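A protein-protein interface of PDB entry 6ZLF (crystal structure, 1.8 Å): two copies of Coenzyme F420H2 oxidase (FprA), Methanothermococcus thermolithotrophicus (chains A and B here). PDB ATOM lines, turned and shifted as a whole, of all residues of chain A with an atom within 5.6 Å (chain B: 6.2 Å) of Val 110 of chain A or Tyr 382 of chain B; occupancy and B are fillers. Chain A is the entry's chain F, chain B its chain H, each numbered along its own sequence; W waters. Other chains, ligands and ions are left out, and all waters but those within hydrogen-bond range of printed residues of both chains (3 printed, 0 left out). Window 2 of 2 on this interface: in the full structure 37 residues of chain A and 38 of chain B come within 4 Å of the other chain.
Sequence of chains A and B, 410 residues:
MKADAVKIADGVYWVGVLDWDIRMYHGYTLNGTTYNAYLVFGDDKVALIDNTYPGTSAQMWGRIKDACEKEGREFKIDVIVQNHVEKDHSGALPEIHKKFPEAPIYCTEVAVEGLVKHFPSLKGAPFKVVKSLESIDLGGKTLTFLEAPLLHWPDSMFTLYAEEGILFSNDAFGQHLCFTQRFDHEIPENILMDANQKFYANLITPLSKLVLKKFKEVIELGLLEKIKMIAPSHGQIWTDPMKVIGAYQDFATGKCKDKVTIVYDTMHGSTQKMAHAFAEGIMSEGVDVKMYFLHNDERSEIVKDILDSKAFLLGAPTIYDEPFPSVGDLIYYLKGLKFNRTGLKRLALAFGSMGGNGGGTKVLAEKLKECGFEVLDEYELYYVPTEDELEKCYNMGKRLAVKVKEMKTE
NZ of Lys 117 of chain A is in salt-bridge range of OE1 of Glu 389 of chain B, at 2.7 Å. The backbone carbonyl oxygen (O) of Val 384 of chain B lies within hydrogen-bond range of the side-chain amino group (NZ) of Lys 117 of chain A, at 2.8 Å. The side-chain amino group (NZ) of Lys 117 of chain A sits at hydrogen-bond distance from the backbone carbonyl oxygen (O) of Tyr 382 of chain B (2.7 Å).
The backbone carbonyl oxygen (O) of Met 354 of chain B is in hydrogen-bond range of the backbone NH (N) of Tyr 383 of chain B. OG1 of Thr 108 of chain A is in hydrogen-bond range of O of Asp 155 of chain A (3.0 Å). The side-chain hydroxyl of Ser 353 of chain B is in hydrogen-bond range of the backbone carbonyl oxygen of Tyr 383 of chain B, at 2.7 Å. The backbone carbonyl oxygen of Gly 355 of chain B sits at hydrogen-bond distance from the side-chain hydroxyl of Tyr 383 of chain B (3.2 Å). The side-chain carboxylate (OD2) of Asp 155 of chain A is in hydrogen-bond range of the backbone NH (N) of Val 85 of chain A (2.9 Å).
Tyr 383 of chain B touches Val 85 of chain A (OH to CG2, 3.7 Å). Val 110 of chain A touches Tyr 382 of chain B (CG2 to OH, 3.99 Å). OH of Tyr 382 of chain B touches CA of Gly 114 of chain A, at 3.9 Å. CA of Gly 114 of chain A touches CE2 of Tyr 383 of chain B, at 3.8 Å. Tyr 383 of chain B touches Asp 155 of chain A.
Printed residues of chain B within 4 Å of Val 85 of chain A: Tyr 383 (3.7 Å). Printed residues of chain B within 4 Å of Val 110 of chain A: Tyr 382 (3.99 Å). Of the printed residues of chain B, Gly 114 of chain A touches Tyr 382 and Tyr 383. Printed residues of chain B within 4 Å of Lys 117 of chain A: Tyr 382 (2.7 Å), Val 384 (2.8 Å) and Glu 389 (2.7 Å). Printed residues of chain B within 4 Å of Asp 155 of chain A: Tyr 383. Gly 352 of chain B touches none of the printed residues of chain A. Of the printed residues of chain A, Tyr 382 of chain B touches Val 110, Gly 114 and Lys 117. The nearest printed residue of chain B that does not touch Val 110 of chain A is Gly 355 of chain B (6.1 Å). The nearest printed residue of chain B that does not touch Lys 117 of chain A is Tyr 383 of chain B (4.1 Å).
Of the 12 printed residues of chain A, 5 touch a printed residue of chain B. Printed residues of chain A that touch a printed residue of chain B: Val 85, Val 110, Gly 114, Lys 117 and Asp 155. Of the 12 printed residues of chain B, 4 touch a printed residue of chain A. Printed residues of chain B that touch a printed residue of chain A: Tyr 382, Tyr 383, Val 384 and Glu 389. Hydrophobic or aromatic side chains of chain B that line the printed part of chain A: Tyr 382, Tyr 383 and Val 384. Among the printed residues, 8 pairs touch across the chains.
No position is printed for both chains. Of the 8 pairs that touch across the chains among the printed residues, none has its exchanged pair printed and touching as well.
Water W3 lies within hydrogen-bond range of the backbone carbonyl oxygen of Lys 117 of chain A (2.6 Å) and the backbone carbonyl oxygen of Val 384 of chain B (3.0 Å). Water W1 lies within hydrogen-bond range of OE2 of Glu 389 of chain B (2.6 Å), N of Tyr 382 of chain B (2.9 Å) and NZ of Lys 117 of chain A (3.5 Å). Water W2 lies within hydrogen-bond range of the side-chain hydroxyl (OH) of Tyr 383 of chain B (2.7 Å), the side-chain carboxylate (OD1) of Asp 155 of chain A (2.8 Å) and the side-chain hydroxyl (OH) of Tyr 382 of chain B (3.5 Å).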
ATOM      1  N   VAL A  85       5.374   3.308   3.111  1.00  0.00           N
ATOM      2  CA  VAL A  85       4.172   4.110   3.398  1.00  0.00           C
ATOM      3  C   VAL A  85       2.864   3.454   2.943  1.00  0.00           C
ATOM      4  O   VAL A  85       1.801   3.916   3.360  1.00  0.00           O
ATOM      5  CB  VAL A  85       4.263   5.561   2.863  1.00  0.00           C
ATOM      6  CG1 VAL A  85       5.584   6.208   3.249  1.00  0.00           C
ATOM      7  CG2 VAL A  85       4.044   5.623   1.363  1.00  0.00           C
ATOM      8  N   THR A 108      11.982   7.010   6.077  1.00  0.00           N
ATOM      9  CA  THR A 108      12.815   7.779   5.145  1.00  0.00           C
ATOM     10  C   THR A 108      12.286   9.210   5.041  1.00  0.00           C
ATOM     11  O   THR A 108      11.169   9.493   5.479  1.00  0.00           O
ATOM     12  CB  THR A 108      12.862   7.117   3.762  1.00  0.00           C
ATOM     13  OG1 THR A 108      11.542   7.089   3.219  1.00  0.00           O
ATOM     14  CG2 THR A 108      13.468   5.714   3.794  1.00  0.00           C
ATOM     15  N   GLU A 109      13.074  10.103   4.437  1.00  0.00           N
ATOM     16  CA  GLU A 109      12.688  11.504   4.276  1.00  0.00           C
ATOM     17  C   GLU A 109      11.403  11.633   3.469  1.00  0.00           C
ATOM     18  O   GLU A 109      10.495  12.339   3.895  1.00  0.00           O
ATOM     19  CB  GLU A 109      13.815  12.295   3.594  1.00  0.00           C
ATOM     20  CG  GLU A 109      13.577  13.795   3.569  1.00  0.00           C
ATOM     21  CD  GLU A 109      14.714  14.611   2.985  1.00  0.00           C
ATOM     22  OE1 GLU A 109      15.760  14.019   2.632  1.00  0.00           O
ATOM     23  OE2 GLU A 109      14.554  15.848   2.872  1.00  0.00           O
ATOM     24  N   VAL A 110      11.323  10.966   2.306  1.00  0.00           N
ATOM     25  CA  VAL A 110      10.125  11.040   1.465  1.00  0.00           C
ATOM     26  C   VAL A 110       8.915  10.363   2.145  1.00  0.00           C
ATOM     27  O   VAL A 110       7.783  10.794   1.926  1.00  0.00           O
ATOM     28  CB  VAL A 110      10.377  10.518   0.019  1.00  0.00           C
ATOM     29  CG1 VAL A 110      10.591   9.012  -0.013  1.00  0.00           C
ATOM     30  CG2 VAL A 110       9.238  10.914  -0.917  1.00  0.00           C
ATOM     31  N   ALA A 111       9.145   9.375   3.023  1.00  0.00           N
ATOM     32  CA  ALA A 111       8.043   8.730   3.745  1.00  0.00           C
ATOM     33  C   ALA A 111       7.253   9.706   4.625  1.00  0.00           C
ATOM     34  O   ALA A 111       6.055   9.527   4.789  1.00  0.00           O
ATOM     35  CB  ALA A 111       8.562   7.597   4.608  1.00  0.00           C
ATOM     36  N   VAL A 112       7.915  10.713   5.224  1.00  0.00           N
ATOM     37  CA  VAL A 112       7.221  11.650   6.115  1.00  0.00           C
ATOM     38  C   VAL A 112       6.066  12.338   5.393  1.00  0.00           C
ATOM     39  O   VAL A 112       4.944  12.341   5.897  1.00  0.00           O
ATOM     40  CB  VAL A 112       8.174  12.700   6.742  1.00  0.00           C
ATOM     41  CG1 VAL A 112       7.395  13.708   7.587  1.00  0.00           C
ATOM     42  CG2 VAL A 112       9.255  12.028   7.583  1.00  0.00           C
ATOM     43  N   GLU A 113       6.337  12.947   4.235  1.00  0.00           N
ATOM     44  CA  GLU A 113       5.289  13.646   3.492  1.00  0.00           C
ATOM     45  C   GLU A 113       4.227  12.669   2.998  1.00  0.00           C
ATOM     46  O   GLU A 113       3.048  12.995   3.035  1.00  0.00           O
ATOM     47  CB  GLU A 113       5.872  14.437   2.309  1.00  0.00           C
ATOM     48  CG  GLU A 113       6.852  15.532   2.711  1.00  0.00           C
ATOM     49  CD  GLU A 113       8.308  15.190   2.458  1.00  0.00           C
ATOM     50  OE1 GLU A 113       8.890  14.450   3.282  1.00  0.00           O
ATOM     51  OE2 GLU A 113       8.854  15.628   1.421  1.00  0.00           O
ATOM     52  N   GLY A 114       4.647  11.479   2.578  1.00  0.00           N
ATOM     53  CA  GLY A 114       3.725  10.443   2.122  1.00  0.00           C
ATOM     54  C   GLY A 114       2.797   9.965   3.220  1.00  0.00           C
ATOM     55  O   GLY A 114       1.596   9.837   2.993  1.00  0.00           O
ATOM     56  N   LEU A 115       3.326   9.762   4.435  1.00  0.00           N
ATOM     57  CA  LEU A 115       2.509   9.311   5.561  1.00  0.00           C
ATOM     58  C   LEU A 115       1.530  10.386   6.030  1.00  0.00           C
ATOM     59  O   LEU A 115       0.373  10.070   6.299  1.00  0.00           O
ATOM     60  CB  LEU A 115       3.388   8.860   6.728  1.00  0.00           C
ATOM     61  CG  LEU A 115       4.156   7.566   6.483  1.00  0.00           C
ATOM     62  CD1 LEU A 115       5.285   7.413   7.475  1.00  0.00           C
ATOM     63  CD2 LEU A 115       3.227   6.353   6.533  1.00  0.00           C
ATOM     64  N   LYS A 117       0.355  12.757   4.125  1.00  0.00           N
ATOM     65  CA  LYS A 117      -0.641  12.869   3.044  1.00  0.00           C
ATOM     66  C   LYS A 117      -1.683  11.742   3.153  1.00  0.00           C
ATOM     67  O   LYS A 117      -2.868  12.012   3.014  1.00  0.00           O
ATOM     68  CB  LYS A 117       0.025  12.868   1.649  1.00  0.00           C
ATOM     69  CG  LYS A 117      -0.844  13.429   0.517  1.00  0.00           C
ATOM     70  CD  LYS A 117      -1.110  14.931   0.672  1.00  0.00           C
ATOM     71  CE  LYS A 117      -1.573  15.627  -0.596  1.00  0.00           C
ATOM     72  NZ  LYS A 117      -2.638  14.885  -1.318  1.00  0.00           N
ATOM     73  N   PRO A 154       9.322   4.857  -3.660  1.00  0.00           N
ATOM     74  CA  PRO A 154      10.454   5.758  -3.332  1.00  0.00           C
ATOM     75  C   PRO A 154      10.796   5.856  -1.838  1.00  0.00           C
ATOM     76  O   PRO A 154      11.918   6.200  -1.478  1.00  0.00           O
ATOM     77  CB  PRO A 154      10.010   7.125  -3.877  1.00  0.00           C
ATOM     78  CG  PRO A 154       8.868   6.860  -4.781  1.00  0.00           C
ATOM     79  CD  PRO A 154       8.237   5.572  -4.363  1.00  0.00           C
ATOM     80  N   ASP A 155       9.802   5.614  -0.979  1.00  0.00           N
ATOM     81  CA  ASP A 155       9.917   5.683   0.483  1.00  0.00           C
ATOM     82  C   ASP A 155      10.485   4.412   1.114  1.00  0.00           C
ATOM     83  O   ASP A 155      10.711   4.398   2.323  1.00  0.00           O
ATOM     84  CB  ASP A 155       8.523   5.917   1.077  1.00  0.00           C
ATOM     85  CG  ASP A 155       7.508   4.937   0.525  1.00  0.00           C
ATOM     86  OD1 ASP A 155       6.923   5.233  -0.536  1.00  0.00           O
ATOM     87  OD2 ASP A 155       7.379   3.832   1.094  1.00  0.00           O
ATOM     88  N   GLY B 352      -6.361  11.251 -11.714  1.00  0.00           N
ATOM     89  CA  GLY B 352      -5.800  10.127 -10.985  1.00  0.00           C
ATOM     90  C   GLY B 352      -4.909  10.513  -9.837  1.00  0.00           C
ATOM     91  O   GLY B 352      -4.494  11.666  -9.708  1.00  0.00           O
ATOM     92  N   SER B 353      -4.615   9.533  -8.995  1.00  0.00           N
ATOM     93  CA  SER B 353      -3.701   9.711  -7.882  1.00  0.00           C
ATOM     94  C   SER B 353      -2.391   8.999  -8.206  1.00  0.00           C
ATOM     95  O   SER B 353      -2.367   8.071  -9.014  1.00  0.00           O
ATOM     96  CB  SER B 353      -4.319   9.158  -6.605  1.00  0.00           C
ATOM     97  OG  SER B 353      -3.444   9.320  -5.504  1.00  0.00           O
ATOM     98  N   MET B 354      -1.297   9.452  -7.605  1.00  0.00           N
ATOM     99  CA  MET B 354       0.008   8.830  -7.818  1.00  0.00           C
ATOM    100  C   MET B 354       0.865   8.993  -6.574  1.00  0.00           C
ATOM    101  O   MET B 354       0.433   9.634  -5.622  1.00  0.00           O
ATOM    102  CB  MET B 354       0.698   9.412  -9.073  1.00  0.00           C
ATOM    103  CG  MET B 354       0.797  10.918  -9.099  1.00  0.00           C
ATOM    104  SD  MET B 354       2.156  11.591  -8.118  1.00  0.00           S
ATOM    105  CE  MET B 354       1.860  13.314  -8.317  1.00  0.00           C
ATOM    106  N   GLY B 355       2.016   8.336  -6.545  1.00  0.00           N
ATOM    107  CA  GLY B 355       2.873   8.349  -5.364  1.00  0.00           C
ATOM    108  C   GLY B 355       4.346   8.584  -5.624  1.00  0.00           C
ATOM    109  O   GLY B 355       5.159   8.381  -4.722  1.00  0.00           O
ATOM    110  N   GLY B 356       4.696   9.034  -6.824  1.00  0.00           N
ATOM    111  CA  GLY B 356       6.089   9.293  -7.173  1.00  0.00           C
ATOM    112  C   GLY B 356       6.224  10.225  -8.358  1.00  0.00           C
ATOM    113  O   GLY B 356       5.850  11.395  -8.263  1.00  0.00           O
ATOM    114  N   GLU B 380      -3.747  15.328 -11.722  1.00  0.00           N
ATOM    115  CA  GLU B 380      -3.096  14.249 -11.004  1.00  0.00           C
ATOM    116  C   GLU B 380      -2.647  14.788  -9.649  1.00  0.00           C
ATOM    117  O   GLU B 380      -2.143  15.909  -9.585  1.00  0.00           O
ATOM    118  CB  GLU B 380      -1.902  13.740 -11.817  1.00  0.00           C
ATOM    119  CG  GLU B 380      -1.397  12.385 -11.378  1.00  0.00           C
ATOM    120  CD  GLU B 380      -0.540  11.681 -12.415  1.00  0.00           C
ATOM    121  OE1 GLU B 380       0.604  12.135 -12.647  1.00  0.00           O
ATOM    122  OE2 GLU B 380      -1.010  10.675 -12.995  1.00  0.00           O
ATOM    123  N   LEU B 381      -2.862  14.024  -8.567  1.00  0.00           N
ATOM    124  CA  LEU B 381      -2.442  14.458  -7.234  1.00  0.00           C
ATOM    125  C   LEU B 381      -1.690  13.348  -6.499  1.00  0.00           C
ATOM    126  O   LEU B 381      -1.629  12.207  -6.966  1.00  0.00           O
ATOM    127  CB  LEU B 381      -3.624  14.997  -6.394  1.00  0.00           C
ATOM    128  CG  LEU B 381      -4.865  14.107  -6.255  1.00  0.00           C
ATOM    129  CD1 LEU B 381      -4.612  12.933  -5.296  1.00  0.00           C
ATOM    130  CD2 LEU B 381      -6.045  14.916  -5.739  1.00  0.00           C
ATOM    131  N   TYR B 382      -1.090  13.706  -5.370  1.00  0.00           N
ATOM    132  CA  TYR B 382      -0.225  12.837  -4.586  1.00  0.00           C
ATOM    133  C   TYR B 382      -1.038  12.090  -3.515  1.00  0.00           C
ATOM    134  O   TYR B 382      -1.631  12.727  -2.649  1.00  0.00           O
ATOM    135  CB  TYR B 382       0.869  13.712  -3.944  1.00  0.00           C
ATOM    136  CG  TYR B 382       1.969  12.966  -3.226  1.00  0.00           C
ATOM    137  CD1 TYR B 382       2.782  12.070  -3.906  1.00  0.00           C
ATOM    138  CD2 TYR B 382       2.331  13.310  -1.929  1.00  0.00           C
ATOM    139  CE1 TYR B 382       3.877  11.474  -3.288  1.00  0.00           C
ATOM    140  CE2 TYR B 382       3.425  12.724  -1.302  1.00  0.00           C
ATOM    141  CZ  TYR B 382       4.205  11.814  -1.990  1.00  0.00           C
ATOM    142  OH  TYR B 382       5.285  11.213  -1.385  1.00  0.00           O
ATOM    143  N   TYR B 383      -1.095  10.751  -3.595  1.00  0.00           N
ATOM    144  CA  TYR B 383      -1.774   9.912  -2.598  1.00  0.00           C
ATOM    145  C   TYR B 383      -3.206  10.382  -2.253  1.00  0.00           C
ATOM    146  O   TYR B 383      -4.010  10.559  -3.170  1.00  0.00           O
ATOM    147  CB  TYR B 383      -0.899   9.762  -1.335  1.00  0.00           C
ATOM    148  CG  TYR B 383       0.406   9.042  -1.593  1.00  0.00           C
ATOM    149  CD1 TYR B 383       0.431   7.826  -2.266  1.00  0.00           C
ATOM    150  CD2 TYR B 383       1.601   9.514  -1.060  1.00  0.00           C
ATOM    151  CE1 TYR B 383       1.616   7.117  -2.434  1.00  0.00           C
ATOM    152  CE2 TYR B 383       2.782   8.792  -1.185  1.00  0.00           C
ATOM    153  CZ  TYR B 383       2.794   7.614  -1.909  1.00  0.00           C
ATOM    154  OH  TYR B 383       3.968   6.927  -2.089  1.00  0.00           O
ATOM    155  N   VAL B 384      -3.538  10.558  -0.961  1.00  0.00           N
ATOM    156  CA  VAL B 384      -4.913  10.810  -0.540  1.00  0.00           C
ATOM    157  C   VAL B 384      -5.265  12.287  -0.745  1.00  0.00           C
ATOM    158  O   VAL B 384      -4.550  13.156  -0.239  1.00  0.00           O
ATOM    159  CB  VAL B 384      -5.130  10.356   0.929  1.00  0.00           C
ATOM    160  CG1 VAL B 384      -6.552  10.646   1.395  1.00  0.00           C
ATOM    161  CG2 VAL B 384      -4.812   8.867   1.088  1.00  0.00           C
ATOM    162  N   PRO B 385      -6.377  12.606  -1.442  1.00  0.00           N
ATOM    163  CA  PRO B 385      -6.718  14.027  -1.642  1.00  0.00           C
ATOM    164  C   PRO B 385      -6.981  14.763  -0.335  1.00  0.00           C
ATOM    165  O   PRO B 385      -7.674  14.236   0.537  1.00  0.00           O
ATOM    166  CB  PRO B 385      -7.987  13.979  -2.509  1.00  0.00           C
ATOM    167  CG  PRO B 385      -8.010  12.628  -3.112  1.00  0.00           C
ATOM    168  CD  PRO B 385      -7.330  11.720  -2.136  1.00  0.00           C
ATOM    169  N   GLU B 389      -7.985  19.756  -2.353  1.00  0.00           N
ATOM    170  CA  GLU B 389      -7.888  19.014  -3.613  1.00  0.00           C
ATOM    171  C   GLU B 389      -9.242  18.451  -4.041  1.00  0.00           C
ATOM    172  O   GLU B 389      -9.550  18.472  -5.228  1.00  0.00           O
ATOM    173  CB  GLU B 389      -6.833  17.911  -3.505  1.00  0.00           C
ATOM    174  CG  GLU B 389      -5.435  18.493  -3.384  1.00  0.00           C
ATOM    175  CD  GLU B 389      -4.333  17.502  -3.087  1.00  0.00           C
ATOM    176  OE1 GLU B 389      -4.584  16.522  -2.350  1.00  0.00           O
ATOM    177  OE2 GLU B 389      -3.191  17.748  -3.532  1.00  0.00           O
HETATM  178  O   HOH W   1      -1.078  16.327  -4.080  1.00  0.00           O
HETATM  179  O   HOH W   2       6.116   7.887  -0.766  1.00  0.00           O
HETATM  180  O   HOH W   3      -4.474  14.011   2.655  1.00  0.00           O
